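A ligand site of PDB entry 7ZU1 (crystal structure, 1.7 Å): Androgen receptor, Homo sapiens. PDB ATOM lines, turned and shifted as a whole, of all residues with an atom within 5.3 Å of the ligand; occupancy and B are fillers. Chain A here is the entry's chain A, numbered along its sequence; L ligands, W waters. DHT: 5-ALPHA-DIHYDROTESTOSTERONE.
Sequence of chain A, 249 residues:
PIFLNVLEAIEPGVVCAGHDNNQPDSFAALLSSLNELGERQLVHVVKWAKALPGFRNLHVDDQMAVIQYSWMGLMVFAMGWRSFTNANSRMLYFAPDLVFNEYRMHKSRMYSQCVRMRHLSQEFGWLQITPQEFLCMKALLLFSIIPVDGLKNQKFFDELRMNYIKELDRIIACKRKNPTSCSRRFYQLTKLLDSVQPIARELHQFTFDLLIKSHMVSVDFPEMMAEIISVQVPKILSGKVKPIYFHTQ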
ATOM      1  N   LEU A  31     -26.819  16.329 -14.356  1.00  0.00           N
ATOM      2  CA  LEU A  31     -27.209  15.317 -13.401  1.00  0.00           C
ATOM      3  C   LEU A  31     -25.990  14.609 -12.802  1.00  0.00           C
ATOM      4  O   LEU A  31     -25.990  14.357 -11.601  1.00  0.00           O
ATOM      5  CB  LEU A  31     -28.235  14.359 -14.026  1.00  0.00           C
ATOM      6  CG  LEU A  31     -29.694  14.693 -13.759  1.00  0.00           C
ATOM      7  CD1 LEU A  31     -30.019  14.593 -12.254  1.00  0.00           C
ATOM      8  CD2 LEU A  31     -30.088  16.071 -14.288  1.00  0.00           C
ATOM      9  N   LEU A  34     -24.877  17.070 -10.258  1.00  0.00           N
ATOM     10  CA  LEU A  34     -25.745  17.049  -9.067  1.00  0.00           C
ATOM     11  C   LEU A  34     -25.452  15.822  -8.202  1.00  0.00           C
ATOM     12  O   LEU A  34     -25.436  15.905  -6.971  1.00  0.00           O
ATOM     13  CB  LEU A  34     -27.210  17.052  -9.495  1.00  0.00           C
ATOM     14  CG  LEU A  34     -27.797  18.416  -9.887  1.00  0.00           C
ATOM     15  CD1 LEU A  34     -29.241  18.214 -10.370  1.00  0.00           C
ATOM     16  CD2 LEU A  34     -27.803  19.352  -8.676  1.00  0.00           C
ATOM     17  N   ASN A  35     -25.196  14.694  -8.865  1.00  0.00           N
ATOM     18  CA  ASN A  35     -24.914  13.433  -8.188  1.00  0.00           C
ATOM     19  C   ASN A  35     -23.598  13.539  -7.414  1.00  0.00           C
ATOM     20  O   ASN A  35     -23.512  13.079  -6.269  1.00  0.00           O
ATOM     21  CB  ASN A  35     -24.807  12.279  -9.173  1.00  0.00           C
ATOM     22  CG  ASN A  35     -26.164  11.781  -9.625  1.00  0.00           C
ATOM     23  OD1 ASN A  35     -27.172  12.065  -8.992  1.00  0.00           O
ATOM     24  ND2 ASN A  35     -26.174  10.995 -10.695  1.00  0.00           N
ATOM     25  N   LEU A  37     -22.214  16.376  -6.387  1.00  0.00           N
ATOM     26  CA  LEU A  37     -22.545  17.258  -5.292  1.00  0.00           C
ATOM     27  C   LEU A  37     -23.196  16.486  -4.132  1.00  0.00           C
ATOM     28  O   LEU A  37     -22.861  16.689  -2.964  1.00  0.00           O
ATOM     29  CB  LEU A  37     -23.418  18.408  -5.807  1.00  0.00           C
ATOM     30  CG  LEU A  37     -23.866  19.374  -4.700  1.00  0.00           C
ATOM     31  CD1 LEU A  37     -22.670  20.116  -4.083  1.00  0.00           C
ATOM     32  CD2 LEU A  37     -24.853  20.382  -5.251  1.00  0.00           C
ATOM     33  N   GLY A  38     -24.138  15.601  -4.453  1.00  0.00           N
ATOM     34  CA  GLY A  38     -24.801  14.789  -3.435  1.00  0.00           C
ATOM     35  C   GLY A  38     -23.788  13.991  -2.605  1.00  0.00           C
ATOM     36  O   GLY A  38     -23.880  13.944  -1.389  1.00  0.00           O
ATOM     37  N   GLN A  41     -21.786  16.379  -0.395  1.00  0.00           N
ATOM     38  CA  GLN A  41     -22.562  16.913   0.712  1.00  0.00           C
ATOM     39  C   GLN A  41     -22.846  15.806   1.720  1.00  0.00           C
ATOM     40  O   GLN A  41     -22.993  16.082   2.894  1.00  0.00           O
ATOM     41  CB  GLN A  41     -23.913  17.446   0.235  1.00  0.00           C
ATOM     42  CG  GLN A  41     -23.719  18.682  -0.626  1.00  0.00           C
ATOM     43  CD  GLN A  41     -24.448  19.835  -0.002  1.00  0.00           C
ATOM     44  OE1 GLN A  41     -25.415  20.338  -0.572  1.00  0.00           O
ATOM     45  NE2 GLN A  41     -23.982  20.231   1.169  1.00  0.00           N
ATOM     46  N   TRP A  71     -31.295  12.124   4.257  1.00  0.00           N
ATOM     47  CA  TRP A  71     -30.334  13.002   3.595  1.00  0.00           C
ATOM     48  C   TRP A  71     -31.008  13.867   2.533  1.00  0.00           C
ATOM     49  O   TRP A  71     -30.617  15.002   2.337  1.00  0.00           O
ATOM     50  CB  TRP A  71     -29.128  12.228   3.001  1.00  0.00           C
ATOM     51  CG  TRP A  71     -29.505  11.245   1.941  1.00  0.00           C
ATOM     52  CD1 TRP A  71     -29.797   9.923   2.136  1.00  0.00           C
ATOM     53  CD2 TRP A  71     -29.598  11.470   0.516  1.00  0.00           C
ATOM     54  NE1 TRP A  71     -30.111   9.324   0.952  1.00  0.00           N
ATOM     55  CE2 TRP A  71     -29.999  10.243  -0.064  1.00  0.00           C
ATOM     56  CE3 TRP A  71     -29.390  12.565  -0.317  1.00  0.00           C
ATOM     57  CZ2 TRP A  71     -30.200  10.100  -1.436  1.00  0.00           C
ATOM     58  CZ3 TRP A  71     -29.607  12.429  -1.676  1.00  0.00           C
ATOM     59  CH2 TRP A  71     -29.991  11.206  -2.224  1.00  0.00           C
ATOM     60  N   MET A  72     -31.976  13.318   1.787  1.00  0.00           N
ATOM     61  CA  MET A  72     -32.531  14.069   0.681  1.00  0.00           C
ATOM     62  C   MET A  72     -33.241  15.321   1.179  1.00  0.00           C
ATOM     63  O   MET A  72     -33.002  16.406   0.668  1.00  0.00           O
ATOM     64  CB  MET A  72     -33.526  13.227  -0.143  1.00  0.00           C
ATOM     65  CG  MET A  72     -34.152  14.025  -1.280  1.00  0.00           C
ATOM     66  SD  MET A  72     -32.982  14.110  -2.688  1.00  0.00           S
ATOM     67  CE  MET A  72     -33.047  12.404  -3.229  1.00  0.00           C
ATOM     68  N   MET A  75     -30.767  17.891   2.545  1.00  0.00           N
ATOM     69  CA  MET A  75     -30.015  18.620   1.511  1.00  0.00           C
ATOM     70  C   MET A  75     -30.916  19.583   0.733  1.00  0.00           C
ATOM     71  O   MET A  75     -30.489  20.704   0.385  1.00  0.00           O
ATOM     72  CB  MET A  75     -29.318  17.685   0.526  1.00  0.00           C
ATOM     73  CG  MET A  75     -28.337  16.735   1.204  1.00  0.00           C
ATOM     74  SD  MET A  75     -27.423  15.843  -0.018  1.00  0.00           S
ATOM     75  CE  MET A  75     -26.497  14.749   1.057  1.00  0.00           C
ATOM     76  N   VAL A  76     -32.148  19.160   0.447  1.00  0.00           N
ATOM     77  CA  VAL A  76     -33.114  20.029  -0.223  1.00  0.00           C
ATOM     78  C   VAL A  76     -33.416  21.269   0.622  1.00  0.00           C
ATOM     79  O   VAL A  76     -33.472  22.383   0.085  1.00  0.00           O
ATOM     80  CB  VAL A  76     -34.391  19.234  -0.560  1.00  0.00           C
ATOM     81  CG1 VAL A  76     -35.559  20.168  -0.888  1.00  0.00           C
ATOM     82  CG2 VAL A  76     -34.099  18.304  -1.709  1.00  0.00           C
ATOM     83  N   MET A  79     -30.562  23.626   0.670  1.00  0.00           N
ATOM     84  CA  MET A  79     -30.376  24.205  -0.646  1.00  0.00           C
ATOM     85  C   MET A  79     -31.408  25.330  -0.825  1.00  0.00           C
ATOM     86  O   MET A  79     -31.060  26.401  -1.349  1.00  0.00           O
ATOM     87  CB  MET A  79     -30.563  23.150  -1.732  1.00  0.00           C
ATOM     88  CG  MET A  79     -30.269  23.634  -3.157  1.00  0.00           C
ATOM     89  SD  MET A  79     -31.663  24.554  -3.914  1.00  0.00           S
ATOM     90  CE  MET A  79     -32.906  23.263  -4.061  1.00  0.00           C
ATOM     91  N   ARG A  82     -29.972  28.268   1.091  1.00  0.00           N
ATOM     92  CA  ARG A  82     -28.896  28.947   0.360  1.00  0.00           C
ATOM     93  C   ARG A  82     -29.458  29.752  -0.809  1.00  0.00           C
ATOM     94  O   ARG A  82     -28.912  30.794  -1.140  1.00  0.00           O
ATOM     95  CB  ARG A  82     -28.015  27.915  -0.358  1.00  0.00           C
ATOM     96  CG  ARG A  82     -27.120  27.132   0.558  1.00  0.00           C
ATOM     97  CD  ARG A  82     -26.030  26.484  -0.306  1.00  0.00           C
ATOM     98  NE  ARG A  82     -26.381  25.341  -1.138  1.00  0.00           N
ATOM     99  CZ  ARG A  82     -26.696  24.141  -0.662  1.00  0.00           C
ATOM    100  NH1 ARG A  82     -26.787  23.925   0.645  1.00  0.00           N
ATOM    101  NH2 ARG A  82     -26.962  23.160  -1.500  1.00  0.00           N
ATOM    102  N   PHE A  94     -27.617  25.302  -5.964  1.00  0.00           N
ATOM    103  CA  PHE A  94     -27.171  23.990  -5.514  1.00  0.00           C
ATOM    104  C   PHE A  94     -25.756  24.095  -4.932  1.00  0.00           C
ATOM    105  O   PHE A  94     -25.508  23.616  -3.830  1.00  0.00           O
ATOM    106  CB  PHE A  94     -27.218  22.970  -6.646  1.00  0.00           C
ATOM    107  CG  PHE A  94     -28.603  22.567  -7.061  1.00  0.00           C
ATOM    108  CD1 PHE A  94     -29.395  21.767  -6.235  1.00  0.00           C
ATOM    109  CD2 PHE A  94     -29.112  22.980  -8.275  1.00  0.00           C
ATOM    110  CE1 PHE A  94     -30.680  21.396  -6.620  1.00  0.00           C
ATOM    111  CE2 PHE A  94     -30.390  22.603  -8.663  1.00  0.00           C
ATOM    112  CZ  PHE A  94     -31.195  21.833  -7.830  1.00  0.00           C
ATOM    113  N   MET A 110     -35.980  18.033 -14.636  1.00  0.00           N
ATOM    114  CA  MET A 110     -36.531  18.016 -13.304  1.00  0.00           C
ATOM    115  C   MET A 110     -37.336  19.294 -13.079  1.00  0.00           C
ATOM    116  O   MET A 110     -37.386  19.783 -11.959  1.00  0.00           O
ATOM    117  CB  MET A 110     -35.447  18.039 -12.212  1.00  0.00           C
ATOM    118  CG  MET A 110     -34.318  17.082 -12.417  1.00  0.00           C
ATOM    119  SD  MET A 110     -33.427  16.880 -10.853  1.00  0.00           S
ATOM    120  CE  MET A 110     -33.700  18.431  -9.992  1.00  0.00           C
ATOM    121  N   MET A 117     -39.077  22.965  -5.312  1.00  0.00           N
ATOM    122  CA  MET A 117     -37.947  23.357  -4.484  1.00  0.00           C
ATOM    123  C   MET A 117     -37.832  24.883  -4.434  1.00  0.00           C
ATOM    124  O   MET A 117     -37.468  25.455  -3.407  1.00  0.00           O
ATOM    125  CB  MET A 117     -36.635  22.765  -5.015  1.00  0.00           C
ATOM    126  CG  MET A 117     -36.526  21.301  -4.740  1.00  0.00           C
ATOM    127  SD  MET A 117     -34.972  20.538  -5.207  1.00  0.00           S
ATOM    128  CE  MET A 117     -35.107  20.410  -6.978  1.00  0.00           C
ATOM    129  N   LEU A 203     -38.138  13.527  -5.429  1.00  0.00           N
ATOM    130  CA  LEU A 203     -36.754  13.415  -5.841  1.00  0.00           C
ATOM    131  C   LEU A 203     -36.237  11.988  -5.644  1.00  0.00           C
ATOM    132  O   LEU A 203     -35.397  11.533  -6.408  1.00  0.00           O
ATOM    133  CB  LEU A 203     -35.936  14.463  -5.069  1.00  0.00           C
ATOM    134  CG  LEU A 203     -36.217  15.907  -5.503  1.00  0.00           C
ATOM    135  CD1 LEU A 203     -35.639  16.874  -4.501  1.00  0.00           C
ATOM    136  CD2 LEU A 203     -35.651  16.190  -6.892  1.00  0.00           C
ATOM    137  N   PHE A 206     -37.446  10.215  -8.589  1.00  0.00           N
ATOM    138  CA  PHE A 206     -36.697  10.662  -9.762  1.00  0.00           C
ATOM    139  C   PHE A 206     -35.311  10.020  -9.791  1.00  0.00           C
ATOM    140  O   PHE A 206     -34.866   9.516 -10.818  1.00  0.00           O
ATOM    141  CB  PHE A 206     -36.579  12.187  -9.736  1.00  0.00           C
ATOM    142  CG  PHE A 206     -35.980  12.756 -10.989  1.00  0.00           C
ATOM    143  CD1 PHE A 206     -34.610  12.904 -11.119  1.00  0.00           C
ATOM    144  CD2 PHE A 206     -36.795  13.077 -12.069  1.00  0.00           C
ATOM    145  CE1 PHE A 206     -34.065  13.389 -12.293  1.00  0.00           C
ATOM    146  CE2 PHE A 206     -36.243  13.533 -13.262  1.00  0.00           C
ATOM    147  CZ  PHE A 206     -34.877  13.692 -13.359  1.00  0.00           C
ATOM    148  N   THR A 207     -34.611  10.061  -8.652  1.00  0.00           N
ATOM    149  CA  THR A 207     -33.237   9.564  -8.617  1.00  0.00           C
ATOM    150  C   THR A 207     -33.180   8.043  -8.767  1.00  0.00           C
ATOM    151  O   THR A 207     -32.254   7.499  -9.378  1.00  0.00           O
ATOM    152  CB  THR A 207     -32.510  10.072  -7.364  1.00  0.00           C
ATOM    153  OG1 THR A 207     -31.113   9.905  -7.600  1.00  0.00           O
ATOM    154  CG2 THR A 207     -32.839   9.308  -6.097  1.00  0.00           C
ATOM    155  N   LEU A 210     -33.629   7.280 -12.296  1.00  0.00           N
ATOM    156  CA  LEU A 210     -32.451   7.666 -13.040  1.00  0.00           C
ATOM    157  C   LEU A 210     -31.320   6.661 -12.844  1.00  0.00           C
ATOM    158  O   LEU A 210     -30.613   6.339 -13.801  1.00  0.00           O
ATOM    159  CB  LEU A 210     -32.043   9.079 -12.601  1.00  0.00           C
ATOM    160  CG  LEU A 210     -30.820   9.671 -13.303  1.00  0.00           C
ATOM    161  CD1 LEU A 210     -30.944   9.592 -14.825  1.00  0.00           C
ATOM    162  CD2 LEU A 210     -30.660  11.109 -12.870  1.00  0.00           C
ATOM    163  N   PHE A 221     -23.212   7.968 -11.345  1.00  0.00           N
ATOM    164  CA  PHE A 221     -23.502   7.953  -9.934  1.00  0.00           C
ATOM    165  C   PHE A 221     -22.238   7.564  -9.174  1.00  0.00           C
ATOM    166  O   PHE A 221     -21.667   6.519  -9.441  1.00  0.00           O
ATOM    167  CB  PHE A 221     -24.645   6.976  -9.653  1.00  0.00           C
ATOM    168  CG  PHE A 221     -26.008   7.502  -9.950  1.00  0.00           C
ATOM    169  CD1 PHE A 221     -26.511   7.475 -11.251  1.00  0.00           C
ATOM    170  CD2 PHE A 221     -26.806   8.028  -8.941  1.00  0.00           C
ATOM    171  CE1 PHE A 221     -27.766   7.999 -11.553  1.00  0.00           C
ATOM    172  CE2 PHE A 221     -28.078   8.518  -9.245  1.00  0.00           C
ATOM    173  CZ  PHE A 221     -28.543   8.517 -10.545  1.00  0.00           C
ATOM    174  N   MET A 225     -23.734   7.233  -3.394  1.00  0.00           N
ATOM    175  CA  MET A 225     -25.021   7.582  -3.964  1.00  0.00           C
ATOM    176  C   MET A 225     -25.684   6.329  -4.540  1.00  0.00           C
ATOM    177  O   MET A 225     -26.803   5.998  -4.167  1.00  0.00           O
ATOM    178  CB  MET A 225     -24.889   8.696  -5.011  1.00  0.00           C
ATOM    179  CG  MET A 225     -24.438  10.035  -4.416  1.00  0.00           C
ATOM    180  SD  MET A 225     -25.745  10.798  -3.378  1.00  0.00           S
ATOM    181  CE  MET A 225     -26.828  11.372  -4.691  1.00  0.00           C
ATOM    182  N   ILE A 229     -29.074   4.779  -2.903  1.00  0.00           N
ATOM    183  CA  ILE A 229     -30.235   4.911  -3.776  1.00  0.00           C
ATOM    184  C   ILE A 229     -30.790   3.515  -4.133  1.00  0.00           C
ATOM    185  O   ILE A 229     -31.999   3.375  -4.327  1.00  0.00           O
ATOM    186  CB  ILE A 229     -29.971   5.808  -5.013  1.00  0.00           C
ATOM    187  CG1 ILE A 229     -29.614   7.225  -4.568  1.00  0.00           C
ATOM    188  CG2 ILE A 229     -31.167   5.787  -5.976  1.00  0.00           C
ATOM    189  CD1 ILE A 229     -29.138   8.127  -5.683  1.00  0.00           C
HETATM  190  C1  DHT L   1     -27.654  17.620  -4.147  1.00  0.00           C
HETATM  191  C2  DHT L   1     -27.507  18.532  -2.921  1.00  0.00           C
HETATM  192  C3  DHT L   1     -28.435  19.713  -3.040  1.00  0.00           C
HETATM  193  O3  DHT L   1     -28.054  20.863  -2.904  1.00  0.00           O
HETATM  194  C4  DHT L   1     -29.866  19.387  -3.334  1.00  0.00           C
HETATM  195  C5  DHT L   1     -30.015  18.393  -4.493  1.00  0.00           C
HETATM  196  C6  DHT L   1     -31.473  18.029  -4.771  1.00  0.00           C
HETATM  197  C7  DHT L   1     -31.562  17.211  -6.054  1.00  0.00           C
HETATM  198  C8  DHT L   1     -30.693  15.949  -5.969  1.00  0.00           C
HETATM  199  C9  DHT L   1     -29.231  16.271  -5.595  1.00  0.00           C
HETATM  200  C10 DHT L   1     -29.115  17.139  -4.321  1.00  0.00           C
HETATM  201  C11 DHT L   1     -28.408  14.983  -5.500  1.00  0.00           C
HETATM  202  C12 DHT L   1     -28.479  14.134  -6.777  1.00  0.00           C
HETATM  203  C13 DHT L   1     -29.935  13.829  -7.137  1.00  0.00           C
HETATM  204  C14 DHT L   1     -30.692  15.158  -7.264  1.00  0.00           C
HETATM  205  C15 DHT L   1     -32.028  14.729  -7.874  1.00  0.00           C
HETATM  206  C16 DHT L   1     -31.601  13.653  -8.901  1.00  0.00           C
HETATM  207  C17 DHT L   1     -30.142  13.316  -8.574  1.00  0.00           C
HETATM  208  O17 DHT L   1     -29.840  11.944  -8.793  1.00  0.00           O
HETATM  209  C18 DHT L   1     -30.580  12.842  -6.140  1.00  0.00           C
HETATM  210  C19 DHT L   1     -29.531  16.347  -3.065  1.00  0.00           C
HETATM  211  O   HOH W   1     -27.673  20.979   0.437  1.00  0.00           O
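OD1 of Asn 35 sits at hydrogen-bond distance from O17 of the ligand (2.7 Å).
The side-chain hydroxyl (OG1) of Thr 207 sits at hydrogen-bond distance from an oxygen (O17) of the ligand (2.7 Å).
The guanidinium group (NH2) of Arg 82 lies within hydrogen-bond range of an oxygen (O3) of the ligand, at 2.9 Å.
The guanidinium group (NH2) of Arg 82 sits at hydrogen-bond distance from the backbone carbonyl oxygen (O) of Phe 94 (2.8 Å).
The side-chain amide oxygen (OE1) of Gln 41 lies within hydrogen-bond range of the guanidinium group (NH2) of Arg 82 (3.3 Å).
The side-chain amide nitrogen of Asn 35 lies close to the backbone carbonyl oxygen of Leu 31, at 3.5 Å.
CD1 of Leu 31 touches C16 of the ligand, at 3.8 Å.
Leu 34 touches the ligand (O to C11, 3.4 Å).
CD2 of Leu 37 touches C2 of the ligand (3.99 Å).
Gln 41 touches the ligand.
Met 72 touches the ligand (CE to C18, 3.8 Å).
Met 75 touches the ligand.
Met 79 touches the ligand (CG to O3, 3.6 Å).
Phe 94 touches the ligand (CD1 to O3, 3.7 Å).
Met 110 touches the ligand.
Phe 206 touches the ligand.
Phe 221 touches the ligand (CE2 to O17, 3.9 Å).
CE of Met 225 touches C12 of the ligand, 3.8 Å away.
Within 4 Å of the ligand: Leu 31, Leu 34, Asn 35, Leu 37, Gln 41, Met 72, Met 75, Met 79, Arg 82, Phe 94, Met 110, Phe 206, Thr 207, Phe 221 and Met 225.
The nearest printed residue that does not touch the ligand is Leu 203 (4.03 Å).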
